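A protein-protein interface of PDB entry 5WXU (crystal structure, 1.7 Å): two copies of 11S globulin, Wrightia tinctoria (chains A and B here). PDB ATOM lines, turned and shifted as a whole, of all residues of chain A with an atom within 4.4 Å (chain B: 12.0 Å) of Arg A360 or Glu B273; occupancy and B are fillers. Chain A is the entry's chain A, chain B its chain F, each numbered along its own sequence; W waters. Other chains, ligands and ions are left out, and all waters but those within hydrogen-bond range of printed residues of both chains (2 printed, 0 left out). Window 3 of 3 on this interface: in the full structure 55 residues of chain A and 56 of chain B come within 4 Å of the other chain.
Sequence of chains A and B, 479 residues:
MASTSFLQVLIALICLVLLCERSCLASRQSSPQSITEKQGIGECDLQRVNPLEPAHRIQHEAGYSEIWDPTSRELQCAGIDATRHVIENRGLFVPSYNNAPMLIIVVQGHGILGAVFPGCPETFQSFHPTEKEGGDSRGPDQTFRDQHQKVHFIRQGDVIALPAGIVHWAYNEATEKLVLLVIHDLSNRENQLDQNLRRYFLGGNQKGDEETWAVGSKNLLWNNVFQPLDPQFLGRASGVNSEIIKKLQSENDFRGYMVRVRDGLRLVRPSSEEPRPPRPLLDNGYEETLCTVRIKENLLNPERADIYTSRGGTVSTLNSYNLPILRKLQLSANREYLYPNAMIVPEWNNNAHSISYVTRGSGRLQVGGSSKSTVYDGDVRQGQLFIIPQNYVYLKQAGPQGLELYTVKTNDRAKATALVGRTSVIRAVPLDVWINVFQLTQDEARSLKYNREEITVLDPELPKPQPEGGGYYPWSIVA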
ATOM      1  N   PRO A 302      15.650 -23.693  20.570  1.00  0.00           N
ATOM      2  CA  PRO A 302      16.696 -24.233  19.624  1.00  0.00           C
ATOM      3  C   PRO A 302      17.254 -23.114  18.773  1.00  0.00           C
ATOM      4  O   PRO A 302      18.377 -23.184  18.329  1.00  0.00           O
ATOM      5  CB  PRO A 302      15.900 -25.227  18.781  1.00  0.00           C
ATOM      6  CG  PRO A 302      14.863 -25.724  19.716  1.00  0.00           C
ATOM      7  CD  PRO A 302      14.396 -24.483  20.467  1.00  0.00           C
ATOM      8  N   THR A 314      22.150 -29.579  19.437  1.00  0.00           N
ATOM      9  CA  THR A 314      22.530 -28.139  19.582  1.00  0.00           C
ATOM     10  C   THR A 314      23.356 -27.974  20.817  1.00  0.00           C
ATOM     11  O   THR A 314      23.206 -28.687  21.805  1.00  0.00           O
ATOM     12  CB  THR A 314      21.321 -27.167  19.728  1.00  0.00           C
ATOM     13  OG1 THR A 314      20.445 -27.568  20.780  1.00  0.00           O
ATOM     14  CG2 THR A 314      20.538 -27.136  18.464  1.00  0.00           C
ATOM     15  N   ARG A 335      23.754 -25.120  27.380  1.00  0.00           N
ATOM     16  CA  ARG A 335      22.769 -26.144  27.291  1.00  0.00           C
ATOM     17  C   ARG A 335      23.111 -27.026  26.075  1.00  0.00           C
ATOM     18  O   ARG A 335      23.316 -26.524  24.992  1.00  0.00           O
ATOM     19  CB  ARG A 335      21.367 -25.553  27.025  1.00  0.00           C
ATOM     20  CG  ARG A 335      20.278 -26.600  26.985  1.00  0.00           C
ATOM     21  CD  ARG A 335      18.944 -25.897  26.757  1.00  0.00           C
ATOM     22  NE  ARG A 335      17.983 -26.845  26.301  1.00  0.00           N
ATOM     23  CZ  ARG A 335      17.727 -27.136  25.029  1.00  0.00           C
ATOM     24  NH1 ARG A 335      18.245 -26.461  24.023  1.00  0.00           N
ATOM     25  NH2 ARG A 335      16.824 -28.062  24.800  1.00  0.00           N
ATOM     26  N   TYR A 337      21.646 -30.305  23.742  1.00  0.00           N
ATOM     27  CA  TYR A 337      20.518 -31.163  23.461  1.00  0.00           C
ATOM     28  C   TYR A 337      20.994 -32.092  22.358  1.00  0.00           C
ATOM     29  O   TYR A 337      21.541 -31.632  21.359  1.00  0.00           O
ATOM     30  CB  TYR A 337      19.348 -30.339  23.036  1.00  0.00           C
ATOM     31  CG  TYR A 337      18.220 -31.252  22.799  1.00  0.00           C
ATOM     32  CD1 TYR A 337      17.427 -31.676  23.858  1.00  0.00           C
ATOM     33  CD2 TYR A 337      18.026 -31.806  21.549  1.00  0.00           C
ATOM     34  CE1 TYR A 337      16.412 -32.617  23.673  1.00  0.00           C
ATOM     35  CE2 TYR A 337      17.031 -32.766  21.345  1.00  0.00           C
ATOM     36  CZ  TYR A 337      16.221 -33.152  22.398  1.00  0.00           C
ATOM     37  OH  TYR A 337      15.217 -34.069  22.183  1.00  0.00           O
ATOM     38  N   TYR A 339      19.848 -35.413  20.059  1.00  0.00           N
ATOM     39  CA  TYR A 339      18.856 -36.392  19.589  1.00  0.00           C
ATOM     40  C   TYR A 339      19.291 -37.796  19.918  1.00  0.00           C
ATOM     41  O   TYR A 339      20.449 -38.040  20.208  1.00  0.00           O
ATOM     42  CB  TYR A 339      18.598 -36.235  18.094  1.00  0.00           C
ATOM     43  CG  TYR A 339      17.873 -34.985  17.822  1.00  0.00           C
ATOM     44  CD1 TYR A 339      16.508 -34.831  18.169  1.00  0.00           C
ATOM     45  CD2 TYR A 339      18.517 -33.922  17.264  1.00  0.00           C
ATOM     46  CE1 TYR A 339      15.844 -33.630  17.932  1.00  0.00           C
ATOM     47  CE2 TYR A 339      17.868 -32.706  17.033  1.00  0.00           C
ATOM     48  CZ  TYR A 339      16.545 -32.548  17.367  1.00  0.00           C
ATOM     49  OH  TYR A 339      15.880 -31.332  17.115  1.00  0.00           O
ATOM     50  N   VAL A 358      21.555 -33.273  34.406  1.00  0.00           N
ATOM     51  CA  VAL A 358      20.693 -33.863  33.356  1.00  0.00           C
ATOM     52  C   VAL A 358      19.245 -33.480  33.575  1.00  0.00           C
ATOM     53  O   VAL A 358      18.649 -33.845  34.565  1.00  0.00           O
ATOM     54  CB  VAL A 358      20.839 -35.386  33.317  1.00  0.00           C
ATOM     55  CG1 VAL A 358      20.074 -35.921  32.142  1.00  0.00           C
ATOM     56  CG2 VAL A 358      22.298 -35.769  33.200  1.00  0.00           C
ATOM     57  N   THR A 359      18.659 -32.722  32.655  1.00  0.00           N
ATOM     58  CA  THR A 359      17.295 -32.271  32.842  1.00  0.00           C
ATOM     59  C   THR A 359      16.290 -33.153  32.129  1.00  0.00           C
ATOM     60  O   THR A 359      15.139 -33.201  32.515  1.00  0.00           O
ATOM     61  CB  THR A 359      17.104 -30.851  32.313  1.00  0.00           C
ATOM     62  OG1 THR A 359      17.706 -30.707  31.011  1.00  0.00           O
ATOM     63  CG2 THR A 359      17.681 -29.893  33.262  1.00  0.00           C
ATOM     64  N   ARG A 360      16.721 -33.847  31.084  1.00  0.00           N
ATOM     65  CA  ARG A 360      15.865 -34.789  30.371  1.00  0.00           C
ATOM     66  C   ARG A 360      16.638 -35.889  29.732  1.00  0.00           C
ATOM     67  O   ARG A 360      17.761 -35.691  29.264  1.00  0.00           O
ATOM     68  CB  ARG A 360      15.168 -34.123  29.192  1.00  0.00           C
ATOM     69  CG  ARG A 360      14.047 -33.163  29.543  1.00  0.00           C
ATOM     70  CD  ARG A 360      13.508 -32.448  28.301  1.00  0.00           C
ATOM     71  NE  ARG A 360      13.386 -33.336  27.148  1.00  0.00           N
ATOM     72  CZ  ARG A 360      13.322 -32.926  25.879  1.00  0.00           C
ATOM     73  NH1 ARG A 360      13.325 -31.618  25.573  1.00  0.00           N
ATOM     74  NH2 ARG A 360      13.243 -33.835  24.893  1.00  0.00           N
ATOM     75  N   GLY A 361      15.990 -37.023  29.633  1.00  0.00           N
ATOM     76  CA  GLY A 361      16.591 -38.132  28.907  1.00  0.00           C
ATOM     77  C   GLY A 361      17.711 -38.834  29.668  1.00  0.00           C
ATOM     78  O   GLY A 361      17.741 -38.904  30.895  1.00  0.00           O
ATOM     79  N   SER A 362      18.663 -39.368  28.907  1.00  0.00           N
ATOM     80  CA  SER A 362      19.722 -40.173  29.443  1.00  0.00           C
ATOM     81  C   SER A 362      20.832 -40.346  28.345  1.00  0.00           C
ATOM     82  O   SER A 362      20.615 -40.093  27.126  1.00  0.00           O
ATOM     83  CB  SER A 362      19.162 -41.532  29.933  1.00  0.00           C
ATOM     84  OG  SER A 362      18.709 -42.256  28.800  1.00  0.00           O
ATOM     85  N   GLN A 382      18.217 -38.269  34.068  1.00  0.00           N
ATOM     86  CA  GLN A 382      17.514 -37.122  34.601  1.00  0.00           C
ATOM     87  C   GLN A 382      17.640 -37.013  36.084  1.00  0.00           C
ATOM     88  O   GLN A 382      17.446 -37.970  36.835  1.00  0.00           O
ATOM     89  CB  GLN A 382      16.019 -37.188  34.219  1.00  0.00           C
ATOM     90  CG  GLN A 382      15.215 -35.975  34.675  1.00  0.00           C
ATOM     91  CD  GLN A 382      13.771 -36.010  34.180  1.00  0.00           C
ATOM     92  OE1 GLN A 382      13.044 -36.930  34.527  1.00  0.00           O
ATOM     93  NE2 GLN A 382      13.344 -35.011  33.400  1.00  0.00           N
ATOM     94  N   LEU A 403      18.926 -36.605  25.098  1.00  0.00           N
ATOM     95  CA  LEU A 403      19.613 -36.141  26.341  1.00  0.00           C
ATOM     96  C   LEU A 403      19.639 -34.621  26.297  1.00  0.00           C
ATOM     97  O   LEU A 403      20.115 -34.032  25.323  1.00  0.00           O
ATOM     98  CB  LEU A 403      21.066 -36.621  26.335  1.00  0.00           C
ATOM     99  CG  LEU A 403      21.920 -36.162  27.555  1.00  0.00           C
ATOM    100  CD1 LEU A 403      21.352 -36.627  28.855  1.00  0.00           C
ATOM    101  CD2 LEU A 403      23.296 -36.677  27.335  1.00  0.00           C
ATOM    102  N   GLU A 404      19.217 -33.990  27.386  1.00  0.00           N
ATOM    103  CA  GLU A 404      19.363 -32.568  27.603  1.00  0.00           C
ATOM    104  C   GLU A 404      20.161 -32.333  28.915  1.00  0.00           C
ATOM    105  O   GLU A 404      19.884 -32.930  29.922  1.00  0.00           O
ATOM    106  CB  GLU A 404      18.038 -31.849  27.674  1.00  0.00           C
ATOM    107  CG  GLU A 404      18.167 -30.323  27.749  1.00  0.00           C
ATOM    108  CD  GLU A 404      16.849 -29.653  28.060  1.00  0.00           C
ATOM    109  OE1 GLU A 404      16.157 -30.125  28.955  1.00  0.00           O
ATOM    110  OE2 GLU A 404      16.435 -28.704  27.380  1.00  0.00           O
ATOM    111  N   THR B 123      29.099 -23.197  11.886  1.00  0.00           N
ATOM    112  CA  THR B 123      28.533 -24.094  12.895  1.00  0.00           C
ATOM    113  C   THR B 123      27.059 -24.434  12.830  1.00  0.00           C
ATOM    114  O   THR B 123      26.593 -25.171  13.696  1.00  0.00           O
ATOM    115  CB  THR B 123      28.822 -23.548  14.301  1.00  0.00           C
ATOM    116  OG1 THR B 123      28.045 -22.355  14.481  1.00  0.00           O
ATOM    117  CG2 THR B 123      30.290 -23.231  14.468  1.00  0.00           C
ATOM    118  N   PHE B 124      26.322 -24.006  11.792  1.00  0.00           N
ATOM    119  CA  PHE B 124      24.962 -24.460  11.505  1.00  0.00           C
ATOM    120  C   PHE B 124      25.143 -25.386  10.294  1.00  0.00           C
ATOM    121  O   PHE B 124      25.518 -24.975   9.228  1.00  0.00           O
ATOM    122  CB  PHE B 124      24.025 -23.311  11.172  1.00  0.00           C
ATOM    123  CG  PHE B 124      23.368 -22.696  12.354  1.00  0.00           C
ATOM    124  CD1 PHE B 124      24.007 -22.640  13.570  1.00  0.00           C
ATOM    125  CD2 PHE B 124      22.070 -22.234  12.279  1.00  0.00           C
ATOM    126  CE1 PHE B 124      23.367 -22.087  14.691  1.00  0.00           C
ATOM    127  CE2 PHE B 124      21.413 -21.716  13.363  1.00  0.00           C
ATOM    128  CZ  PHE B 124      22.082 -21.641  14.599  1.00  0.00           C
ATOM    129  N   GLN B 125      24.980 -26.660  10.549  1.00  0.00           N
ATOM    130  CA  GLN B 125      25.436 -27.741   9.678  1.00  0.00           C
ATOM    131  C   GLN B 125      24.352 -28.762   9.385  1.00  0.00           C
ATOM    132  O   GLN B 125      23.722 -29.278  10.298  1.00  0.00           O
ATOM    133  CB  GLN B 125      26.546 -28.459  10.421  1.00  0.00           C
ATOM    134  CG  GLN B 125      27.710 -27.583  10.893  1.00  0.00           C
ATOM    135  CD  GLN B 125      28.463 -28.249  12.046  1.00  0.00           C
ATOM    136  OE1 GLN B 125      29.382 -28.974  11.824  1.00  0.00           O
ATOM    137  NE2 GLN B 125      28.033 -28.016  13.269  1.00  0.00           N
ATOM    138  N   LYS B 150      25.795 -18.987  12.038  1.00  0.00           N
ATOM    139  CA  LYS B 150      24.570 -18.830  12.791  1.00  0.00           C
ATOM    140  C   LYS B 150      23.644 -17.856  12.132  1.00  0.00           C
ATOM    141  O   LYS B 150      24.073 -16.804  11.670  1.00  0.00           O
ATOM    142  CB  LYS B 150      24.889 -18.320  14.215  1.00  0.00           C
ATOM    143  CG  LYS B 150      23.651 -18.000  15.030  1.00  0.00           C
ATOM    144  CD  LYS B 150      23.939 -17.855  16.520  1.00  0.00           C
ATOM    145  CE  LYS B 150      22.629 -17.875  17.294  1.00  0.00           C
ATOM    146  NZ  LYS B 150      22.830 -18.080  18.747  1.00  0.00           N
ATOM    147  N   PHE B 153      16.982 -15.191  14.597  1.00  0.00           N
ATOM    148  CA  PHE B 153      15.576 -15.093  14.416  1.00  0.00           C
ATOM    149  C   PHE B 153      15.162 -13.776  15.070  1.00  0.00           C
ATOM    150  O   PHE B 153      15.290 -13.582  16.303  1.00  0.00           O
ATOM    151  CB  PHE B 153      14.922 -16.322  14.963  1.00  0.00           C
ATOM    152  CG  PHE B 153      15.426 -17.579  14.251  1.00  0.00           C
ATOM    153  CD1 PHE B 153      16.626 -18.195  14.621  1.00  0.00           C
ATOM    154  CD2 PHE B 153      14.807 -18.021  13.109  1.00  0.00           C
ATOM    155  CE1 PHE B 153      17.154 -19.286  13.923  1.00  0.00           C
ATOM    156  CE2 PHE B 153      15.322 -19.138  12.389  1.00  0.00           C
ATOM    157  CZ  PHE B 153      16.501 -19.745  12.785  1.00  0.00           C
ATOM    158  N   VAL B 268      19.678 -23.845   7.042  1.00  0.00           N
ATOM    159  CA  VAL B 268      19.941 -24.863   7.985  1.00  0.00           C
ATOM    160  C   VAL B 268      19.570 -24.218   9.312  1.00  0.00           C
ATOM    161  O   VAL B 268      20.154 -23.233   9.680  1.00  0.00           O
ATOM    162  CB  VAL B 268      21.435 -25.215   8.022  1.00  0.00           C
ATOM    163  CG1 VAL B 268      21.709 -26.239   9.102  1.00  0.00           C
ATOM    164  CG2 VAL B 268      21.889 -25.761   6.663  1.00  0.00           C
ATOM    165  N   ARG B 269      18.534 -24.705   9.967  1.00  0.00           N
ATOM    166  CA  ARG B 269      18.002 -24.003  11.123  1.00  0.00           C
ATOM    167  C   ARG B 269      17.543 -25.059  12.096  1.00  0.00           C
ATOM    168  O   ARG B 269      17.007 -26.122  11.660  1.00  0.00           O
ATOM    169  CB  ARG B 269      16.868 -23.036  10.766  1.00  0.00           C
ATOM    170  CG  ARG B 269      15.575 -23.660  10.317  1.00  0.00           C
ATOM    171  CD  ARG B 269      14.524 -22.568  10.053  1.00  0.00           C
ATOM    172  NE  ARG B 269      14.338 -22.291   8.620  1.00  0.00           N
ATOM    173  CZ  ARG B 269      13.520 -21.355   8.119  1.00  0.00           C
ATOM    174  NH1 ARG B 269      12.791 -20.562   8.920  1.00  0.00           N
ATOM    175  NH2 ARG B 269      13.428 -21.208   6.802  1.00  0.00           N
ATOM    176  N   PRO B 270      17.800 -24.809  13.399  1.00  0.00           N
ATOM    177  CA  PRO B 270      17.544 -25.769  14.430  1.00  0.00           C
ATOM    178  C   PRO B 270      16.096 -26.217  14.401  1.00  0.00           C
ATOM    179  O   PRO B 270      15.169 -25.399  14.305  1.00  0.00           O
ATOM    180  CB  PRO B 270      17.868 -25.015  15.734  1.00  0.00           C
ATOM    181  CG  PRO B 270      18.869 -24.023  15.330  1.00  0.00           C
ATOM    182  CD  PRO B 270      18.523 -23.620  13.918  1.00  0.00           C
ATOM    183  N   SER B 271      15.977 -27.538  14.452  1.00  0.00           N
ATOM    184  CA  SER B 271      14.767 -28.280  14.540  1.00  0.00           C
ATOM    185  C   SER B 271      14.227 -28.296  15.992  1.00  0.00           C
ATOM    186  O   SER B 271      14.958 -28.047  16.964  1.00  0.00           O
ATOM    187  CB  SER B 271      15.139 -29.719  14.148  1.00  0.00           C
ATOM    188  OG  SER B 271      16.300 -30.151  14.937  1.00  0.00           O
ATOM    189  N   SER B 272      12.954 -28.650  16.114  1.00  0.00           N
ATOM    190  CA  SER B 272      12.306 -28.778  17.424  1.00  0.00           C
ATOM    191  C   SER B 272      12.954 -29.896  18.271  1.00  0.00           C
ATOM    192  O   SER B 272      13.359 -30.966  17.753  1.00  0.00           O
ATOM    193  CB  SER B 272      10.808 -29.026  17.242  1.00  0.00           C
ATOM    194  OG  SER B 272      10.196 -29.466  18.453  1.00  0.00           O
ATOM    195  N   GLU B 273      13.000 -29.645  19.575  1.00  0.00           N
ATOM    196  CA  GLU B 273      13.620 -30.557  20.557  1.00  0.00           C
ATOM    197  C   GLU B 273      12.587 -30.973  21.645  1.00  0.00           C
ATOM    198  O   GLU B 273      12.847 -30.796  22.834  1.00  0.00           O
ATOM    199  CB  GLU B 273      14.827 -29.851  21.186  1.00  0.00           C
ATOM    200  CG  GLU B 273      15.913 -29.438  20.168  1.00  0.00           C
ATOM    201  CD  GLU B 273      17.100 -28.635  20.747  1.00  0.00           C
ATOM    202  OE1 GLU B 273      16.933 -27.982  21.812  1.00  0.00           O
ATOM    203  OE2 GLU B 273      18.175 -28.635  20.078  1.00  0.00           O
ATOM    204  N   GLU B 274      11.415 -31.492  21.237  1.00  0.00           N
ATOM    205  CA  GLU B 274      10.455 -32.142  22.185  1.00  0.00           C
ATOM    206  C   GLU B 274      10.745 -33.645  22.316  1.00  0.00           C
ATOM    207  O   GLU B 274       9.961 -34.398  22.905  1.00  0.00           O
ATOM    208  CB  GLU B 274       8.972 -31.967  21.775  1.00  0.00           C
ATOM    209  CG  GLU B 274       8.555 -30.647  21.138  1.00  0.00           C
ATOM    210  CD  GLU B 274       8.878 -29.418  21.970  1.00  0.00           C
ATOM    211  OE1 GLU B 274       9.457 -29.523  23.080  1.00  0.00           O
ATOM    212  OE2 GLU B 274       8.542 -28.317  21.493  1.00  0.00           O
HETATM  213  O   HOH W   1      17.517 -28.897  17.159  1.00  0.00           O
HETATM  214  O   HOH W   2      14.090 -29.222  25.570  1.00  0.00           O
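OG of Ser B271 is in hydrogen-bond range of OH of Tyr A339, at 2.5 Å. The guanidinium group of Arg A335 lies within salt-bridge range of the side-chain carboxylate of Glu B273, at 3.0 Å. The side-chain hydroxyl (OG1) of Thr A314 is in hydrogen-bond range of the side-chain carboxylate (OE2) of Glu B273 (2.6 Å). O of Ser B272 is in hydrogen-bond range of OH of Tyr A339, at 2.6 Å. The guanidinium group (NH1) of Arg A360 is in hydrogen-bond range of the backbone carbonyl oxygen (O) of Glu B273, at 2.9 Å.
NH2 of Arg A360 lies within hydrogen-bond range of OH of Tyr A337, 3.4 Å away. The guanidinium group (NE) of Arg A335 lies within salt-bridge range of the side-chain carboxylate (OE2) of Glu A404, 2.6 Å away. The backbone carbonyl oxygen of Tyr A337 is in hydrogen-bond range of the backbone NH of Thr A314 (2.9 Å). The backbone carbonyl oxygen (O) of Arg A360 is in hydrogen-bond range of the backbone NH (N) of Glu A404, 2.9 Å away.
Pro A302 touches Pro B270 (O to CG, 3.2 Å). Pro A302 touches Ser B271. Pro A302 touches Glu B273 (CG to OE1, 3.7 Å). Glu B273 touches Tyr A337 (CD to CD2, 3.4 Å). Glu B273 touches Tyr A339. Arg A360 touches Glu B274.
Of chain B, only Glu B273 and Glu B274 come within 4 Å of Arg A360. Pro A302 touches three residues of chain B. Of chain B, only Glu B273 (3.4 Å) comes within 4 Å of Tyr A337. No residue of chain B comes within 4 Å of Val A358. No residue of chain B comes within 4 Å of Gly A361. No residue of chain B comes within 4 Å of Ser A362. No residue of chain B comes within 4 Å of Gln A382. Of the printed residues of chain B, Tyr A339 touches Ser B271 (2.5 Å), Ser B272 (2.6 Å) and Glu B273 (3.6 Å). Printed residues of chain A within 4 Å of Ser B272: Tyr A339. Printed residues of chain A within 4 Å of Ser B271: Pro A302 and Tyr A339. Printed residues of chain A within 4 Å of Pro B270: Pro A302 (3.2 Å). Thr B123 touches none of the printed residues of chain A. Lys B150 touches none of the printed residues of chain A. The nearest residue of chain B that does not touch Arg A360 is Ser B272 (7.5 Å). The nearest printed residue of chain A that does not touch Glu B273 is Glu A404 (5.6 Å).
Printed residues of chain B that touch a printed residue of chain A: Pro B270, Ser B271, Ser B272, Glu B273 and Glu B274. Printed residues of chain A that touch a printed residue of chain B: Pro A302, Thr A314, Arg A335, Tyr A337, Tyr A339 and Arg A360. Hydrophobic or aromatic side chains of chain A within 4 Å of the printed part of chain B: Pro A302, Tyr A337 and Tyr A339. Among the printed residues, 11 pairs touch across the chains.
No position is printed for both chains. Of the 11 pairs that touch across the chains among the printed residues, none has its exchanged pair printed and touching as well.
Water W2 lies within hydrogen-bond range of the guanidinium group of Arg A360, the side-chain carboxylate of Glu A404, the guanidinium group of Arg A335 and the backbone carbonyl oxygen of Glu B273. Water W1 lies within hydrogen-bond range of the backbone carbonyl oxygen (O) of Ser B271 (2.7 Å), the side-chain hydroxyl (OH) of Tyr A339 (2.9 Å) and the side-chain carboxylate (OE2) of Glu B273 (3.0 Å).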
